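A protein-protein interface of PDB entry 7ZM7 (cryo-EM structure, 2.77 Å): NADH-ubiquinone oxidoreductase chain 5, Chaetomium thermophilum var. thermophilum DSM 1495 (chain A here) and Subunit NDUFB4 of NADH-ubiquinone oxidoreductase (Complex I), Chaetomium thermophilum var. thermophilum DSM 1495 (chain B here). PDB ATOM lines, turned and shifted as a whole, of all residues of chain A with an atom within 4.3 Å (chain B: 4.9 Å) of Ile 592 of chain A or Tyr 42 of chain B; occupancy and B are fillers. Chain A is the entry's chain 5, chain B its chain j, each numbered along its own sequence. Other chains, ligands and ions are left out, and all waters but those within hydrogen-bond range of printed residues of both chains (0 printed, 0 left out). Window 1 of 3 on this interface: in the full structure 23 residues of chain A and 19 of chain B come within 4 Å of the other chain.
The backbone NH (N) of Asp 597 of chain A lies within hydrogen-bond range of the backbone carbonyl oxygen (O) of Ile 592 of chain A (2.9 Å).
CD2 of Leu 588 of chain A touches OH of Tyr 42 of chain B (3.2 Å).
CG2 of Val 38 of chain B touches NE2 of Gln 591 of chain A (3.9 Å).
OE1 of Gln 591 of chain A touches OH of Tyr 42 of chain B, at 3.5 Å.
CG1 of Ile 592 of chain A touches CE1 of Tyr 42 of chain B (3.7 Å).
Leu 596 of chain A touches Val 38 of chain B.
Leu 596 of chain A touches Ser 39 of chain B (CD2 to CA, 3.98 Å).
CD1 of Leu 596 of chain A touches CB of Tyr 42 of chain B (3.6 Å).
Of the printed residues of chain B, Gln 591 of chain A touches Val 38 (3.9 Å) and Tyr 42 (3.5 Å).
Printed residues of chain B within 4 Å of Ile 592 of chain A: Tyr 42 (3.7 Å).
Of the printed residues of chain B, Leu 596 of chain A touches Val 38 (3.7 Å), Ser 39 (3.98 Å) and Tyr 42 (3.6 Å).
Printed residues of chain A within 4 Å of Val 38 of chain B: Gln 591 and Leu 596.
Of the printed residues of chain A, Ser 39 of chain B touches Leu 596.
Tyr 42 of chain B touches just these residues of chain A: Leu 588 (3.2 Å), Gln 591 (3.5 Å), Ile 592 (3.7 Å) and Leu 596 (3.6 Å).
The nearest printed residue of chain A that does not touch Tyr 42 of chain B is Gly 589 of chain A (5.6 Å).
Printed residues of chain A that touch a printed residue of chain B: Leu 588, Gln 591, Ile 592 and Leu 596.
Among the printed residues, no Asp or Glu carboxylate lies within 4 Å of a Lys or Arg side-chain nitrogen of the other chain.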
ATOM      1  N   LEU A 588      -2.119 -10.114 -23.004  1.00  0.00           N
ATOM      2  CA  LEU A 588      -0.887  -9.932 -22.250  1.00  0.00           C
ATOM      3  C   LEU A 588       0.082  -9.052 -23.016  1.00  0.00           C
ATOM      4  O   LEU A 588       0.697  -8.148 -22.445  1.00  0.00           O
ATOM      5  CB  LEU A 588      -0.231 -11.275 -21.944  1.00  0.00           C
ATOM      6  CG  LEU A 588      -0.816 -12.242 -20.917  1.00  0.00           C
ATOM      7  CD1 LEU A 588       0.099 -13.426 -20.803  1.00  0.00           C
ATOM      8  CD2 LEU A 588      -0.990 -11.612 -19.575  1.00  0.00           C
ATOM      9  N   GLY A 589       0.222  -9.295 -24.314  1.00  0.00           N
ATOM     10  CA  GLY A 589       1.075  -8.449 -25.121  1.00  0.00           C
ATOM     11  C   GLY A 589       0.583  -7.022 -25.180  1.00  0.00           C
ATOM     12  O   GLY A 589       1.383  -6.083 -25.195  1.00  0.00           O
ATOM     13  N   GLY A 590      -0.735  -6.837 -25.217  1.00  0.00           N
ATOM     14  CA  GLY A 590      -1.287  -5.497 -25.184  1.00  0.00           C
ATOM     15  C   GLY A 590      -1.068  -4.800 -23.857  1.00  0.00           C
ATOM     16  O   GLY A 590      -0.787  -3.604 -23.815  1.00  0.00           O
ATOM     17  N   GLN A 591      -1.213  -5.534 -22.758  1.00  0.00           N
ATOM     18  CA  GLN A 591      -1.020  -4.948 -21.436  1.00  0.00           C
ATOM     19  C   GLN A 591       0.422  -4.518 -21.223  1.00  0.00           C
ATOM     20  O   GLN A 591       0.683  -3.453 -20.655  1.00  0.00           O
ATOM     21  CB  GLN A 591      -1.453  -5.941 -20.361  1.00  0.00           C
ATOM     22  CG  GLN A 591      -2.885  -5.762 -19.960  1.00  0.00           C
ATOM     23  CD  GLN A 591      -3.151  -6.154 -18.535  1.00  0.00           C
ATOM     24  OE1 GLN A 591      -2.378  -6.887 -17.924  1.00  0.00           O
ATOM     25  NE2 GLN A 591      -4.252  -5.660 -17.987  1.00  0.00           N
ATOM     26  N   ILE A 592       1.371  -5.337 -21.674  1.00  0.00           N
ATOM     27  CA  ILE A 592       2.778  -4.979 -21.564  1.00  0.00           C
ATOM     28  C   ILE A 592       3.095  -3.780 -22.442  1.00  0.00           C
ATOM     29  O   ILE A 592       3.857  -2.894 -22.047  1.00  0.00           O
ATOM     30  CB  ILE A 592       3.663  -6.191 -21.902  1.00  0.00           C
ATOM     31  CG1 ILE A 592       3.374  -7.331 -20.930  1.00  0.00           C
ATOM     32  CG2 ILE A 592       5.121  -5.822 -21.809  1.00  0.00           C
ATOM     33  CD1 ILE A 592       3.944  -8.619 -21.323  1.00  0.00           C
ATOM     34  N   THR A 593       2.527  -3.732 -23.646  1.00  0.00           N
ATOM     35  CA  THR A 593       2.785  -2.612 -24.546  1.00  0.00           C
ATOM     36  C   THR A 593       2.181  -1.319 -24.020  1.00  0.00           C
ATOM     37  O   THR A 593       2.839  -0.273 -24.018  1.00  0.00           O
ATOM     38  CB  THR A 593       2.244  -2.915 -25.945  1.00  0.00           C
ATOM     39  OG1 THR A 593       2.763  -4.159 -26.415  1.00  0.00           O
ATOM     40  CG2 THR A 593       2.637  -1.818 -26.915  1.00  0.00           C
ATOM     41  N   LYS A 594       0.925  -1.359 -23.584  1.00  0.00           N
ATOM     42  CA  LYS A 594       0.248  -0.119 -23.225  1.00  0.00           C
ATOM     43  C   LYS A 594       0.558   0.315 -21.801  1.00  0.00           C
ATOM     44  O   LYS A 594       0.932   1.463 -21.564  1.00  0.00           O
ATOM     45  CB  LYS A 594      -1.261  -0.252 -23.405  1.00  0.00           C
ATOM     46  CG  LYS A 594      -1.705  -0.477 -24.816  1.00  0.00           C
ATOM     47  CD  LYS A 594      -3.230  -0.513 -24.874  1.00  0.00           C
ATOM     48  CE  LYS A 594      -3.860  -1.750 -24.247  1.00  0.00           C
ATOM     49  NZ  LYS A 594      -3.539  -2.983 -24.996  1.00  0.00           N
ATOM     50  N   LEU A 596       2.851  -0.740 -19.581  1.00  0.00           N
ATOM     51  CA  LEU A 596       4.218  -0.713 -19.086  1.00  0.00           C
ATOM     52  C   LEU A 596       5.166   0.011 -20.025  1.00  0.00           C
ATOM     53  O   LEU A 596       5.738   1.030 -19.635  1.00  0.00           O
ATOM     54  CB  LEU A 596       4.731  -2.134 -18.825  1.00  0.00           C
ATOM     55  CG  LEU A 596       3.780  -3.148 -18.197  1.00  0.00           C
ATOM     56  CD1 LEU A 596       4.481  -4.446 -18.016  1.00  0.00           C
ATOM     57  CD2 LEU A 596       3.257  -2.670 -16.884  1.00  0.00           C
ATOM     58  N   ASP A 597       5.327  -0.465 -21.260  1.00  0.00           N
ATOM     59  CA  ASP A 597       6.313   0.123 -22.166  1.00  0.00           C
ATOM     60  C   ASP A 597       6.030   1.588 -22.404  1.00  0.00           C
ATOM     61  O   ASP A 597       6.940   2.419 -22.416  1.00  0.00           O
ATOM     62  CB  ASP A 597       6.314  -0.600 -23.508  1.00  0.00           C
ATOM     63  CG  ASP A 597       6.854  -1.987 -23.418  1.00  0.00           C
ATOM     64  OD1 ASP A 597       7.704  -2.231 -22.547  1.00  0.00           O
ATOM     65  OD2 ASP A 597       6.432  -2.840 -24.206  1.00  0.00           O
ATOM     66  N   VAL B  38      -0.989  -3.555 -12.244  1.00  0.00           N
ATOM     67  CA  VAL B  38      -0.286  -4.190 -13.353  1.00  0.00           C
ATOM     68  C   VAL B  38       1.206  -3.865 -13.292  1.00  0.00           C
ATOM     69  O   VAL B  38       2.058  -4.740 -13.484  1.00  0.00           O
ATOM     70  CB  VAL B  38      -0.916  -3.761 -14.692  1.00  0.00           C
ATOM     71  CG1 VAL B  38      -0.031  -4.127 -15.845  1.00  0.00           C
ATOM     72  CG2 VAL B  38      -2.283  -4.373 -14.856  1.00  0.00           C
ATOM     73  N   SER B  39       1.543  -2.611 -12.991  1.00  0.00           N
ATOM     74  CA  SER B  39       2.945  -2.209 -12.947  1.00  0.00           C
ATOM     75  C   SER B  39       3.680  -2.887 -11.803  1.00  0.00           C
ATOM     76  O   SER B  39       4.911  -2.896 -11.764  1.00  0.00           O
ATOM     77  CB  SER B  39       3.053  -0.691 -12.814  1.00  0.00           C
ATOM     78  OG  SER B  39       2.380  -0.040 -13.873  1.00  0.00           O
ATOM     79  N   PHE B  40       2.949  -3.437 -10.846  1.00  0.00           N
ATOM     80  CA  PHE B  40       3.605  -4.104  -9.731  1.00  0.00           C
ATOM     81  C   PHE B  40       3.747  -5.593  -9.987  1.00  0.00           C
ATOM     82  O   PHE B  40       4.741  -6.205  -9.587  1.00  0.00           O
ATOM     83  CB  PHE B  40       2.832  -3.846  -8.444  1.00  0.00           C
ATOM     84  CG  PHE B  40       3.333  -4.618  -7.275  1.00  0.00           C
ATOM     85  CD1 PHE B  40       4.460  -4.214  -6.596  1.00  0.00           C
ATOM     86  CD2 PHE B  40       2.684  -5.763  -6.866  1.00  0.00           C
ATOM     87  CE1 PHE B  40       4.914  -4.924  -5.536  1.00  0.00           C
ATOM     88  CE2 PHE B  40       3.135  -6.463  -5.799  1.00  0.00           C
ATOM     89  CZ  PHE B  40       4.252  -6.049  -5.135  1.00  0.00           C
ATOM     90  N   MET B  41       2.754  -6.195 -10.635  1.00  0.00           N
ATOM     91  CA  MET B  41       2.792  -7.630 -10.873  1.00  0.00           C
ATOM     92  C   MET B  41       3.839  -7.991 -11.915  1.00  0.00           C
ATOM     93  O   MET B  41       4.643  -8.906 -11.715  1.00  0.00           O
ATOM     94  CB  MET B  41       1.411  -8.109 -11.304  1.00  0.00           C
ATOM     95  CG  MET B  41       0.351  -7.975 -10.234  1.00  0.00           C
ATOM     96  SD  MET B  41       0.747  -8.948  -8.777  1.00  0.00           S
ATOM     97  CE  MET B  41       0.540 -10.600  -9.432  1.00  0.00           C
ATOM     98  N   TYR B  42       3.845  -7.275 -13.035  1.00  0.00           N
ATOM     99  CA  TYR B  42       4.762  -7.591 -14.118  1.00  0.00           C
ATOM    100  C   TYR B  42       6.201  -7.264 -13.754  1.00  0.00           C
ATOM    101  O   TYR B  42       7.125  -7.976 -14.151  1.00  0.00           O
ATOM    102  CB  TYR B  42       4.383  -6.815 -15.369  1.00  0.00           C
ATOM    103  CG  TYR B  42       3.308  -7.400 -16.237  1.00  0.00           C
ATOM    104  CD1 TYR B  42       3.538  -8.541 -16.973  1.00  0.00           C
ATOM    105  CD2 TYR B  42       2.103  -6.745 -16.404  1.00  0.00           C
ATOM    106  CE1 TYR B  42       2.574  -9.049 -17.794  1.00  0.00           C
ATOM    107  CE2 TYR B  42       1.143  -7.231 -17.231  1.00  0.00           C
ATOM    108  CZ  TYR B  42       1.374  -8.384 -17.929  1.00  0.00           C
ATOM    109  OH  TYR B  42       0.401  -8.882 -18.764  1.00  0.00           O
ATOM    110  N   VAL B  43       6.418  -6.160 -13.051  1.00  0.00           N
ATOM    111  CA  VAL B  43       7.779  -5.696 -12.847  1.00  0.00           C
ATOM    112  C   VAL B  43       8.418  -6.330 -11.620  1.00  0.00           C
ATOM    113  O   VAL B  43       9.626  -6.575 -11.612  1.00  0.00           O
ATOM    114  CB  VAL B  43       7.808  -4.164 -12.763  1.00  0.00           C
ATOM    115  CG1 VAL B  43       9.199  -3.689 -12.518  1.00  0.00           C
ATOM    116  CG2 VAL B  43       7.283  -3.567 -14.047  1.00  0.00           C
ATOM    117  N   VAL B  44       7.637  -6.637 -10.600  1.00  0.00           N
ATOM    118  CA  VAL B  44       8.161  -7.099  -9.327  1.00  0.00           C
ATOM    119  C   VAL B  44       7.829  -8.564  -9.095  1.00  0.00           C
ATOM    120  O   VAL B  44       8.722  -9.394  -8.959  1.00  0.00           O
ATOM    121  CB  VAL B  44       7.651  -6.216  -8.168  1.00  0.00           C
ATOM    122  CG1 VAL B  44       8.115  -6.758  -6.842  1.00  0.00           C
ATOM    123  CG2 VAL B  44       8.085  -4.776  -8.372  1.00  0.00           C
ATOM    124  N   VAL B  46       6.274 -11.209 -10.829  1.00  0.00           N
ATOM    125  CA  VAL B  46       6.680 -12.237 -11.786  1.00  0.00           C
ATOM    126  C   VAL B  46       8.194 -12.384 -11.867  1.00  0.00           C
ATOM    127  O   VAL B  46       8.678 -13.526 -11.901  1.00  0.00           O
ATOM    128  CB  VAL B  46       6.039 -11.964 -13.158  1.00  0.00           C
ATOM    129  CG1 VAL B  46       6.452 -13.012 -14.151  1.00  0.00           C
ATOM    130  CG2 VAL B  46       4.538 -11.928 -13.037  1.00  0.00           C
ATOM    131  N   PRO B  47       8.989 -11.311 -11.937  1.00  0.00           N
ATOM    132  CA  PRO B  47      10.440 -11.509 -11.956  1.00  0.00           C
ATOM    133  C   PRO B  47      11.005 -11.948 -10.623  1.00  0.00           C
ATOM    134  O   PRO B  47      11.978 -12.707 -10.596  1.00  0.00           O
ATOM    135  CB  PRO B  47      10.965 -10.136 -12.386  1.00  0.00           C
ATOM    136  CG  PRO B  47       9.849  -9.470 -12.983  1.00  0.00           C
ATOM    137  CD  PRO B  47       8.656  -9.921 -12.263  1.00  0.00           C
